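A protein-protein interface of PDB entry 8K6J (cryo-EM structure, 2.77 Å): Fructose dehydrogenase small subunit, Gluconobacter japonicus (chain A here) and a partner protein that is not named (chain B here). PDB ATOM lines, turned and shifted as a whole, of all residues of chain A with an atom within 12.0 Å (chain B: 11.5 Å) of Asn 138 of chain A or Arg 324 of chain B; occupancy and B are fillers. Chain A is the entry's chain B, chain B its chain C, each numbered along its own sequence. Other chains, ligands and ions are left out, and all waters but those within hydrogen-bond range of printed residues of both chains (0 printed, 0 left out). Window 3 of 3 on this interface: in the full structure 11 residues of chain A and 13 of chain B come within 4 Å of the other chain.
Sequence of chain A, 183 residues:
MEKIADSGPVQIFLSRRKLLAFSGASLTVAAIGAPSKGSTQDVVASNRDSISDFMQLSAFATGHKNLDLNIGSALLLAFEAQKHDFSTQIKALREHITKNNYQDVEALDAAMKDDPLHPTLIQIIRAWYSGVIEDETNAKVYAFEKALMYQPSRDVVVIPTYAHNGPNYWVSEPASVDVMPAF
O of Asn 138 of chain A is in hydrogen-bond range of NH2 of Arg 324 of chain B. NH1 of Arg 324 of chain B is in hydrogen-bond range of O of Ala 139 of chain A. The backbone carbonyl oxygen (O) of Val 141 of chain A sits at hydrogen-bond distance from the side-chain amide nitrogen (ND2) of Asn 321 of chain B (2.8 Å).
O of Gly 131 of chain A sits at hydrogen-bond distance from N of Tyr 142 of chain A (2.8 Å). The backbone carbonyl oxygen (O) of Ala 318 of chain B sits at hydrogen-bond distance from the side-chain amide nitrogen (ND2) of Asn 321 of chain B. O of Asn 321 of chain B lies within hydrogen-bond range of NE of Arg 324 of chain B (3.4 Å).
Asn 138 of chain A touches one residue of chain B. Arg 324 of chain B touches just these residues of chain A: Asn 138 (2.9 Å) and Ala 139 (3.1 Å). Printed residues of chain B within 4 Å of Ala 139 of chain A: Arg 324 (3.1 Å). Lys 140 of chain A touches just one residue of chain B: Asn 321. Of chain B, only Val 317, Ala 318 and Asn 321 come within 4 Å of Val 141 of chain A. Of chain A, only Lys 140 (3.4 Å) and Val 141 (2.8 Å) come within 4 Å of Asn 321 of chain B. No residue of chain A comes within 4 Å of Ser 322 of chain B. No residue of chain A comes within 4 Å of Ser 325 of chain B. No residue of chain A comes within 4 Å of Asn 326 of chain B. Of the printed residues of chain A, Val 317 of chain B touches Val 141 and Tyr 142. Printed residues of chain B within 4 Å of Tyr 142 of chain A: Val 317 and Ala 318. Of the printed residues of chain A, Ala 318 of chain B touches Val 141 (3.9 Å) and Tyr 142 (3.6 Å). The nearest residue of chain B that does not touch Asn 138 of chain A is Asn 321 of chain B (6.2 Å). The nearest residue of chain A that does not touch Arg 324 of chain B is Lys 140 of chain A (4.1 Å).
CB of Lys 140 of chain A touches ND2 of Asn 321 of chain B, 3.4 Å away. O of Val 141 of chain A touches O of Val 317 of chain B, at 3.8 Å. Ala 318 of chain B touches Val 141 of chain A. Tyr 142 of chain A touches Val 317 of chain B (O to CB, 3.96 Å). Tyr 142 of chain A touches Ala 318 of chain B.
Hydrophobic or aromatic side chains of chain A that line the printed part of chain B: Tyr 142. Of the 20 printed residues of chain B, 4 touch a printed residue of chain A. Hydrophobic or aromatic side chains of chain B that line the printed part of chain A: Val 317 and Ala 318. Among the printed residues, 8 pairs touch across the chains. Among the printed residues, no Asp or Glu carboxylate lies within 4 Å of a Lys or Arg side-chain nitrogen of the other chain.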
ATOM      1  N   ALA A  78      29.094  -8.505  18.311  1.00  0.00           N
ATOM      2  CA  ALA A  78      28.336  -9.446  19.128  1.00  0.00           C
ATOM      3  C   ALA A  78      29.259 -10.402  19.874  1.00  0.00           C
ATOM      4  O   ALA A  78      29.010 -10.734  21.038  1.00  0.00           O
ATOM      5  CB  ALA A  78      27.354 -10.218  18.252  1.00  0.00           C
ATOM      6  N   GLN A  82      29.646 -10.865  23.864  1.00  0.00           N
ATOM      7  CA  GLN A  82      29.437 -12.148  24.527  1.00  0.00           C
ATOM      8  C   GLN A  82      30.680 -12.589  25.293  1.00  0.00           C
ATOM      9  O   GLN A  82      30.574 -13.097  26.415  1.00  0.00           O
ATOM     10  CB  GLN A  82      29.021 -13.200  23.499  1.00  0.00           C
ATOM     11  CG  GLN A  82      29.618 -14.577  23.713  1.00  0.00           C
ATOM     12  CD  GLN A  82      28.935 -15.640  22.876  1.00  0.00           C
ATOM     13  OE1 GLN A  82      27.720 -15.823  22.953  1.00  0.00           O
ATOM     14  NE2 GLN A  82      29.716 -16.349  22.070  1.00  0.00           N
ATOM     15  N   SER A 130      25.510 -19.910   9.762  1.00  0.00           N
ATOM     16  CA  SER A 130      24.105 -19.862  10.144  1.00  0.00           C
ATOM     17  C   SER A 130      23.588 -18.453  10.381  1.00  0.00           C
ATOM     18  O   SER A 130      22.391 -18.209  10.208  1.00  0.00           O
ATOM     19  CB  SER A 130      23.874 -20.695  11.407  1.00  0.00           C
ATOM     20  OG  SER A 130      24.368 -20.024  12.550  1.00  0.00           O
ATOM     21  N   GLY A 131      24.453 -17.523  10.768  1.00  0.00           N
ATOM     22  CA  GLY A 131      24.039 -16.164  11.033  1.00  0.00           C
ATOM     23  C   GLY A 131      23.676 -15.867  12.469  1.00  0.00           C
ATOM     24  O   GLY A 131      23.270 -14.736  12.763  1.00  0.00           O
ATOM     25  N   VAL A 132      23.805 -16.837  13.372  1.00  0.00           N
ATOM     26  CA  VAL A 132      23.520 -16.637  14.784  1.00  0.00           C
ATOM     27  C   VAL A 132      24.685 -17.171  15.600  1.00  0.00           C
ATOM     28  O   VAL A 132      25.455 -18.022  15.150  1.00  0.00           O
ATOM     29  CB  VAL A 132      22.211 -17.322  15.226  1.00  0.00           C
ATOM     30  CG1 VAL A 132      21.020 -16.608  14.640  1.00  0.00           C
ATOM     31  CG2 VAL A 132      22.218 -18.779  14.815  1.00  0.00           C
ATOM     32  N   ILE A 133      24.807 -16.656  16.822  1.00  0.00           N
ATOM     33  CA  ILE A 133      25.822 -17.118  17.749  1.00  0.00           C
ATOM     34  C   ILE A 133      25.236 -17.947  18.886  1.00  0.00           C
ATOM     35  O   ILE A 133      25.891 -18.886  19.353  1.00  0.00           O
ATOM     36  CB  ILE A 133      26.629 -15.930  18.307  1.00  0.00           C
ATOM     37  CG1 ILE A 133      25.680 -14.839  18.801  1.00  0.00           C
ATOM     38  CG2 ILE A 133      27.552 -15.375  17.243  1.00  0.00           C
ATOM     39  CD1 ILE A 133      26.352 -13.520  19.047  1.00  0.00           C
ATOM     40  N   GLU A 134      24.029 -17.633  19.343  1.00  0.00           N
ATOM     41  CA  GLU A 134      23.391 -18.326  20.449  1.00  0.00           C
ATOM     42  C   GLU A 134      22.387 -19.350  19.933  1.00  0.00           C
ATOM     43  O   GLU A 134      21.874 -19.245  18.817  1.00  0.00           O
ATOM     44  CB  GLU A 134      22.692 -17.328  21.373  1.00  0.00           C
ATOM     45  CG  GLU A 134      23.594 -16.237  21.908  1.00  0.00           C
ATOM     46  CD  GLU A 134      22.855 -14.935  22.126  1.00  0.00           C
ATOM     47  OE1 GLU A 134      22.039 -14.865  23.068  1.00  0.00           O
ATOM     48  OE2 GLU A 134      23.087 -13.982  21.353  1.00  0.00           O
ATOM     49  N   ASP A 135      22.110 -20.347  20.769  1.00  0.00           N
ATOM     50  CA  ASP A 135      21.190 -21.420  20.423  1.00  0.00           C
ATOM     51  C   ASP A 135      19.762 -21.155  20.881  1.00  0.00           C
ATOM     52  O   ASP A 135      18.879 -21.974  20.612  1.00  0.00           O
ATOM     53  CB  ASP A 135      21.680 -22.745  21.014  1.00  0.00           C
ATOM     54  CG  ASP A 135      23.185 -22.902  20.923  1.00  0.00           C
ATOM     55  OD1 ASP A 135      23.813 -22.177  20.124  1.00  0.00           O
ATOM     56  OD2 ASP A 135      23.741 -23.747  21.654  1.00  0.00           O
ATOM     57  N   GLU A 136      19.513 -20.038  21.558  1.00  0.00           N
ATOM     58  CA  GLU A 136      18.174 -19.723  22.024  1.00  0.00           C
ATOM     59  C   GLU A 136      17.281 -19.308  20.857  1.00  0.00           C
ATOM     60  O   GLU A 136      17.741 -19.042  19.744  1.00  0.00           O
ATOM     61  CB  GLU A 136      18.206 -18.617  23.084  1.00  0.00           C
ATOM     62  CG  GLU A 136      19.045 -18.875  24.353  1.00  0.00           C
ATOM     63  CD  GLU A 136      20.551 -18.982  24.136  1.00  0.00           C
ATOM     64  OE1 GLU A 136      21.298 -18.689  25.091  1.00  0.00           O
ATOM     65  OE2 GLU A 136      21.001 -19.361  23.036  1.00  0.00           O
ATOM     66  N   THR A 137      15.978 -19.257  21.127  1.00  0.00           N
ATOM     67  CA  THR A 137      14.996 -18.901  20.112  1.00  0.00           C
ATOM     68  C   THR A 137      14.882 -17.400  19.890  1.00  0.00           C
ATOM     69  O   THR A 137      14.284 -16.984  18.893  1.00  0.00           O
ATOM     70  CB  THR A 137      13.625 -19.462  20.491  1.00  0.00           C
ATOM     71  OG1 THR A 137      12.613 -18.835  19.694  1.00  0.00           O
ATOM     72  CG2 THR A 137      13.339 -19.205  21.962  1.00  0.00           C
ATOM     73  N   ASN A 138      15.426 -16.582  20.787  1.00  0.00           N
ATOM     74  CA  ASN A 138      15.433 -15.136  20.626  1.00  0.00           C
ATOM     75  C   ASN A 138      16.792 -14.596  20.198  1.00  0.00           C
ATOM     76  O   ASN A 138      17.011 -13.383  20.256  1.00  0.00           O
ATOM     77  CB  ASN A 138      14.933 -14.459  21.914  1.00  0.00           C
ATOM     78  CG  ASN A 138      15.959 -14.460  23.057  1.00  0.00           C
ATOM     79  OD1 ASN A 138      17.171 -14.536  22.857  1.00  0.00           O
ATOM     80  ND2 ASN A 138      15.451 -14.372  24.279  1.00  0.00           N
ATOM     81  N   ALA A 139      17.703 -15.470  19.779  1.00  0.00           N
ATOM     82  CA  ALA A 139      19.029 -15.033  19.369  1.00  0.00           C
ATOM     83  C   ALA A 139      18.939 -14.124  18.152  1.00  0.00           C
ATOM     84  O   ALA A 139      18.134 -14.348  17.245  1.00  0.00           O
ATOM     85  CB  ALA A 139      19.911 -16.242  19.059  1.00  0.00           C
ATOM     86  N   LYS A 140      19.763 -13.082  18.144  1.00  0.00           N
ATOM     87  CA  LYS A 140      19.775 -12.151  17.027  1.00  0.00           C
ATOM     88  C   LYS A 140      20.314 -12.830  15.777  1.00  0.00           C
ATOM     89  O   LYS A 140      21.304 -13.563  15.826  1.00  0.00           O
ATOM     90  CB  LYS A 140      20.625 -10.929  17.365  1.00  0.00           C
ATOM     91  CG  LYS A 140      20.258 -10.268  18.680  1.00  0.00           C
ATOM     92  CD  LYS A 140      20.366  -8.758  18.589  1.00  0.00           C
ATOM     93  CE  LYS A 140      19.567  -8.090  19.691  1.00  0.00           C
ATOM     94  NZ  LYS A 140      19.821  -8.726  21.012  1.00  0.00           N
ATOM     95  N   VAL A 141      19.654 -12.584  14.651  1.00  0.00           N
ATOM     96  CA  VAL A 141      20.086 -13.092  13.355  1.00  0.00           C
ATOM     97  C   VAL A 141      20.867 -11.986  12.665  1.00  0.00           C
ATOM     98  O   VAL A 141      20.352 -10.878  12.476  1.00  0.00           O
ATOM     99  CB  VAL A 141      18.897 -13.546  12.498  1.00  0.00           C
ATOM    100  CG1 VAL A 141      19.309 -13.656  11.047  1.00  0.00           C
ATOM    101  CG2 VAL A 141      18.371 -14.869  12.992  1.00  0.00           C
ATOM    102  N   TYR A 142      22.110 -12.278  12.292  1.00  0.00           N
ATOM    103  CA  TYR A 142      22.971 -11.286  11.671  1.00  0.00           C
ATOM    104  C   TYR A 142      23.131 -11.483  10.171  1.00  0.00           C
ATOM    105  O   TYR A 142      23.727 -10.625   9.515  1.00  0.00           O
ATOM    106  CB  TYR A 142      24.352 -11.296  12.336  1.00  0.00           C
ATOM    107  CG  TYR A 142      24.309 -10.929  13.800  1.00  0.00           C
ATOM    108  CD1 TYR A 142      24.403  -9.608  14.205  1.00  0.00           C
ATOM    109  CD2 TYR A 142      24.172 -11.904  14.774  1.00  0.00           C
ATOM    110  CE1 TYR A 142      24.360  -9.269  15.539  1.00  0.00           C
ATOM    111  CE2 TYR A 142      24.129 -11.575  16.110  1.00  0.00           C
ATOM    112  CZ  TYR A 142      24.221 -10.256  16.486  1.00  0.00           C
ATOM    113  OH  TYR A 142      24.178  -9.921  17.818  1.00  0.00           O
ATOM    114  N   ALA A 143      22.612 -12.576   9.614  1.00  0.00           N
ATOM    115  CA  ALA A 143      22.777 -12.837   8.188  1.00  0.00           C
ATOM    116  C   ALA A 143      21.710 -13.824   7.738  1.00  0.00           C
ATOM    117  O   ALA A 143      21.705 -14.975   8.183  1.00  0.00           O
ATOM    118  CB  ALA A 143      24.173 -13.373   7.898  1.00  0.00           C
ATOM    119  N   PHE A 144      20.818 -13.372   6.863  1.00  0.00           N
ATOM    120  CA  PHE A 144      19.897 -14.241   6.145  1.00  0.00           C
ATOM    121  C   PHE A 144      19.989 -13.915   4.664  1.00  0.00           C
ATOM    122  O   PHE A 144      20.173 -12.753   4.290  1.00  0.00           O
ATOM    123  CB  PHE A 144      18.457 -14.077   6.629  1.00  0.00           C
ATOM    124  CG  PHE A 144      17.483 -14.983   5.935  1.00  0.00           C
ATOM    125  CD1 PHE A 144      17.677 -16.352   5.928  1.00  0.00           C
ATOM    126  CD2 PHE A 144      16.377 -14.468   5.289  1.00  0.00           C
ATOM    127  CE1 PHE A 144      16.784 -17.186   5.291  1.00  0.00           C
ATOM    128  CE2 PHE A 144      15.482 -15.300   4.651  1.00  0.00           C
ATOM    129  CZ  PHE A 144      15.687 -16.660   4.653  1.00  0.00           C
ATOM    130  N   TYR B 315      20.534  -2.978   3.010  1.00  0.00           N
ATOM    131  CA  TYR B 315      20.143  -2.796   4.396  1.00  0.00           C
ATOM    132  C   TYR B 315      21.003  -3.673   5.303  1.00  0.00           C
ATOM    133  O   TYR B 315      21.866  -4.426   4.848  1.00  0.00           O
ATOM    134  CB  TYR B 315      18.651  -3.092   4.563  1.00  0.00           C
ATOM    135  CG  TYR B 315      18.291  -4.511   4.952  1.00  0.00           C
ATOM    136  CD1 TYR B 315      18.711  -5.596   4.197  1.00  0.00           C
ATOM    137  CD2 TYR B 315      17.491  -4.756   6.060  1.00  0.00           C
ATOM    138  CE1 TYR B 315      18.375  -6.885   4.555  1.00  0.00           C
ATOM    139  CE2 TYR B 315      17.144  -6.039   6.420  1.00  0.00           C
ATOM    140  CZ  TYR B 315      17.586  -7.100   5.665  1.00  0.00           C
ATOM    141  OH  TYR B 315      17.241  -8.382   6.024  1.00  0.00           O
ATOM    142  N   SER B 316      20.770  -3.570   6.606  1.00  0.00           N
ATOM    143  CA  SER B 316      21.475  -4.367   7.600  1.00  0.00           C
ATOM    144  C   SER B 316      20.486  -5.320   8.252  1.00  0.00           C
ATOM    145  O   SER B 316      19.471  -4.883   8.805  1.00  0.00           O
ATOM    146  CB  SER B 316      22.136  -3.474   8.650  1.00  0.00           C
ATOM    147  OG  SER B 316      23.150  -4.173   9.347  1.00  0.00           O
ATOM    148  N   VAL B 317      20.780  -6.619   8.181  1.00  0.00           N
ATOM    149  CA  VAL B 317      19.914  -7.610   8.809  1.00  0.00           C
ATOM    150  C   VAL B 317      19.966  -7.481  10.325  1.00  0.00           C
ATOM    151  O   VAL B 317      18.959  -7.680  11.014  1.00  0.00           O
ATOM    152  CB  VAL B 317      20.303  -9.025   8.348  1.00  0.00           C
ATOM    153  CG1 VAL B 317      19.283 -10.037   8.831  1.00  0.00           C
ATOM    154  CG2 VAL B 317      20.429  -9.071   6.839  1.00  0.00           C
ATOM    155  N   ALA B 318      21.140  -7.147  10.866  1.00  0.00           N
ATOM    156  CA  ALA B 318      21.305  -7.086  12.315  1.00  0.00           C
ATOM    157  C   ALA B 318      20.415  -6.019  12.935  1.00  0.00           C
ATOM    158  O   ALA B 318      19.858  -6.221  14.019  1.00  0.00           O
ATOM    159  CB  ALA B 318      22.770  -6.830  12.662  1.00  0.00           C
ATOM    160  N   ASN B 319      20.272  -4.872  12.269  1.00  0.00           N
ATOM    161  CA  ASN B 319      19.450  -3.798  12.810  1.00  0.00           C
ATOM    162  C   ASN B 319      17.979  -4.177  12.898  1.00  0.00           C
ATOM    163  O   ASN B 319      17.239  -3.558  13.668  1.00  0.00           O
ATOM    164  CB  ASN B 319      19.606  -2.537  11.963  1.00  0.00           C
ATOM    165  CG  ASN B 319      20.996  -1.948  12.048  1.00  0.00           C
ATOM    166  OD1 ASN B 319      21.856  -2.461  12.761  1.00  0.00           O
ATOM    167  ND2 ASN B 319      21.224  -0.864  11.319  1.00  0.00           N
ATOM    168  N   ALA B 320      17.538  -5.174  12.132  1.00  0.00           N
ATOM    169  CA  ALA B 320      16.139  -5.574  12.134  1.00  0.00           C
ATOM    170  C   ALA B 320      15.768  -6.441  13.328  1.00  0.00           C
ATOM    171  O   ALA B 320      14.578  -6.697  13.537  1.00  0.00           O
ATOM    172  CB  ALA B 320      15.802  -6.321  10.844  1.00  0.00           C
ATOM    173  N   ASN B 321      16.750  -6.896  14.109  1.00  0.00           N
ATOM    174  CA  ASN B 321      16.451  -7.761  15.245  1.00  0.00           C
ATOM    175  C   ASN B 321      15.624  -7.032  16.294  1.00  0.00           C
ATOM    176  O   ASN B 321      14.715  -7.616  16.895  1.00  0.00           O
ATOM    177  CB  ASN B 321      17.748  -8.285  15.855  1.00  0.00           C
ATOM    178  CG  ASN B 321      18.334  -9.430  15.067  1.00  0.00           C
ATOM    179  OD1 ASN B 321      17.674 -10.439  14.838  1.00  0.00           O
ATOM    180  ND2 ASN B 321      19.579  -9.278  14.640  1.00  0.00           N
ATOM    181  N   SER B 322      15.924  -5.754  16.531  1.00  0.00           N
ATOM    182  CA  SER B 322      15.170  -4.981  17.508  1.00  0.00           C
ATOM    183  C   SER B 322      13.716  -4.794  17.102  1.00  0.00           C
ATOM    184  O   SER B 322      12.875  -4.528  17.966  1.00  0.00           O
ATOM    185  CB  SER B 322      15.825  -3.618  17.715  1.00  0.00           C
ATOM    186  OG  SER B 322      15.773  -2.847  16.528  1.00  0.00           O
ATOM    187  N   ARG B 323      13.401  -4.932  15.818  1.00  0.00           N
ATOM    188  CA  ARG B 323      12.049  -4.731  15.320  1.00  0.00           C
ATOM    189  C   ARG B 323      11.228  -6.010  15.308  1.00  0.00           C
ATOM    190  O   ARG B 323      10.118  -6.012  14.769  1.00  0.00           O
ATOM    191  CB  ARG B 323      12.090  -4.129  13.915  1.00  0.00           C
ATOM    192  CG  ARG B 323      12.154  -2.616  13.903  1.00  0.00           C
ATOM    193  CD  ARG B 323      11.968  -2.072  12.504  1.00  0.00           C
ATOM    194  NE  ARG B 323      12.722  -2.834  11.519  1.00  0.00           N
ATOM    195  CZ  ARG B 323      13.963  -2.554  11.147  1.00  0.00           C
ATOM    196  NH1 ARG B 323      14.628  -1.541  11.674  1.00  0.00           N
ATOM    197  NH2 ARG B 323      14.550  -3.310  10.227  1.00  0.00           N
ATOM    198  N   ARG B 324      11.750  -7.099  15.861  1.00  0.00           N
ATOM    199  CA  ARG B 324      10.935  -8.288  16.038  1.00  0.00           C
ATOM    200  C   ARG B 324       9.940  -8.068  17.171  1.00  0.00           C
ATOM    201  O   ARG B 324      10.091  -7.165  17.998  1.00  0.00           O
ATOM    202  CB  ARG B 324      11.812  -9.504  16.321  1.00  0.00           C
ATOM    203  CG  ARG B 324      12.740  -9.858  15.179  1.00  0.00           C
ATOM    204  CD  ARG B 324      13.533 -11.108  15.486  1.00  0.00           C
ATOM    205  NE  ARG B 324      14.322 -10.959  16.701  1.00  0.00           N
ATOM    206  CZ  ARG B 324      15.286 -11.787  17.070  1.00  0.00           C
ATOM    207  NH1 ARG B 324      15.617 -12.835  16.335  1.00  0.00           N
ATOM    208  NH2 ARG B 324      15.936 -11.559  18.209  1.00  0.00           N
ATOM    209  N   SER B 325       8.903  -8.904  17.196  1.00  0.00           N
ATOM    210  CA  SER B 325       7.784  -8.738  18.123  1.00  0.00           C
ATOM    211  C   SER B 325       7.134  -7.368  17.963  1.00  0.00           C
ATOM    212  O   SER B 325       6.617  -6.795  18.925  1.00  0.00           O
ATOM    213  CB  SER B 325       8.218  -8.955  19.575  1.00  0.00           C
ATOM    214  OG  SER B 325       8.777  -7.768  20.111  1.00  0.00           O
ATOM    215  N   ASN B 326       7.160  -6.837  16.742  1.00  0.00           N
ATOM    216  CA  ASN B 326       6.714  -5.480  16.449  1.00  0.00           C
ATOM    217  C   ASN B 326       5.849  -5.491  15.188  1.00  0.00           C
ATOM    218  O   ASN B 326       6.089  -4.744  14.240  1.00  0.00           O
ATOM    219  CB  ASN B 326       7.912  -4.545  16.303  1.00  0.00           C
ATOM    220  CG  ASN B 326       7.510  -3.098  16.121  1.00  0.00           C
ATOM    221  OD1 ASN B 326       8.288  -2.287  15.623  1.00  0.00           O
ATOM    222  ND2 ASN B 326       6.294  -2.763  16.529  1.00  0.00           N
ATOM    223  N   SER B 327       4.849  -6.373  15.168  1.00  0.00           N
ATOM    224  CA  SER B 327       3.926  -6.471  14.040  1.00  0.00           C
ATOM    225  C   SER B 327       3.292  -5.123  13.732  1.00  0.00           C
ATOM    226  O   SER B 327       3.321  -4.208  14.560  1.00  0.00           O
ATOM    227  CB  SER B 327       2.835  -7.498  14.345  1.00  0.00           C
ATOM    228  OG  SER B 327       1.662  -6.860  14.816  1.00  0.00           O
ATOM    229  N   THR B 328       2.702  -5.010  12.535  1.00  0.00           N
ATOM    230  CA  THR B 328       2.137  -3.750  12.061  1.00  0.00           C
ATOM    231  C   THR B 328       3.265  -2.721  11.989  1.00  0.00           C
ATOM    232  O   THR B 328       3.455  -1.914  12.904  1.00  0.00           O
ATOM    233  CB  THR B 328       0.955  -3.304  12.940  1.00  0.00           C
ATOM    234  OG1 THR B 328      -0.209  -4.033  12.542  1.00  0.00           O
ATOM    235  CG2 THR B 328       0.615  -1.834  12.728  1.00  0.00           C
ATOM    236  N   LEU B 329       4.098  -2.825  10.952  1.00  0.00           N
ATOM    237  CA  LEU B 329       5.364  -2.094  10.897  1.00  0.00           C
ATOM    238  C   LEU B 329       5.081  -0.595  10.802  1.00  0.00           C
ATOM    239  O   LEU B 329       4.830  -0.022   9.739  1.00  0.00           O
ATOM    240  CB  LEU B 329       6.230  -2.587   9.736  1.00  0.00           C
ATOM    241  CG  LEU B 329       5.998  -2.288   8.243  1.00  0.00           C
ATOM    242  CD1 LEU B 329       6.989  -3.049   7.382  1.00  0.00           C
ATOM    243  CD2 LEU B 329       4.579  -2.590   7.797  1.00  0.00           C
ATOM    244  N   THR B 330       5.100   0.047  11.966  1.00  0.00           N
ATOM    245  CA  THR B 330       5.052   1.498  12.060  1.00  0.00           C
ATOM    246  C   THR B 330       6.360   2.094  12.548  1.00  0.00           C
ATOM    247  O   THR B 330       6.647   3.259  12.255  1.00  0.00           O
ATOM    248  CB  THR B 330       3.922   1.935  12.996  1.00  0.00           C
ATOM    249  OG1 THR B 330       3.948   1.135  14.182  1.00  0.00           O
ATOM    250  CG2 THR B 330       2.574   1.769  12.313  1.00  0.00           C
ATOM    251  N   LYS B 331       7.157   1.323  13.283  1.00  0.00           N
ATOM    252  CA  LYS B 331       8.477   1.748  13.722  1.00  0.00           C
ATOM    253  C   LYS B 331       9.556   1.468  12.688  1.00  0.00           C
ATOM    254  O   LYS B 331      10.718   1.819  12.915  1.00  0.00           O
ATOM    255  CB  LYS B 331       8.840   1.063  15.042  1.00  0.00           C
ATOM    256  CG  LYS B 331       7.693   0.992  16.034  1.00  0.00           C
ATOM    257  CD  LYS B 331       8.157   1.351  17.435  1.00  0.00           C
ATOM    258  CE  LYS B 331       7.460   0.500  18.480  1.00  0.00           C
ATOM    259  NZ  LYS B 331       6.054   0.198  18.102  1.00  0.00           N
ATOM    260  N   THR B 332       9.205   0.844  11.566  1.00  0.00           N
ATOM    261  CA  THR B 332      10.160   0.584  10.490  1.00  0.00           C
ATOM    262  C   THR B 332      10.218   1.801   9.566  1.00  0.00           C
ATOM    263  O   THR B 332       9.716   1.804   8.442  1.00  0.00           O
ATOM    264  CB  THR B 332       9.778  -0.678   9.730  1.00  0.00           C
ATOM    265  OG1 THR B 332       9.297  -1.662  10.652  1.00  0.00           O
ATOM    266  CG2 THR B 332      10.981  -1.233   8.988  1.00  0.00           C
ATOM    267  N   ALA B 337      15.140  -0.894   5.097  1.00  0.00           N
ATOM    268  CA  ALA B 337      14.390  -1.959   5.752  1.00  0.00           C
ATOM    269  C   ALA B 337      13.000  -2.102   5.150  1.00  0.00           C
ATOM    270  O   ALA B 337      12.512  -3.220   4.958  1.00  0.00           O
ATOM    271  CB  ALA B 337      14.299  -1.691   7.252  1.00  0.00           C
ATOM    272  N   ALA B 341      11.596  -5.439   3.326  1.00  0.00           N
ATOM    273  CA  ALA B 341      10.415  -6.136   3.817  1.00  0.00           C
ATOM    274  C   ALA B 341       9.343  -6.241   2.741  1.00  0.00           C
ATOM    275  O   ALA B 341       8.700  -7.287   2.602  1.00  0.00           O
ATOM    276  CB  ALA B 341       9.866  -5.430   5.054  1.00  0.00           C
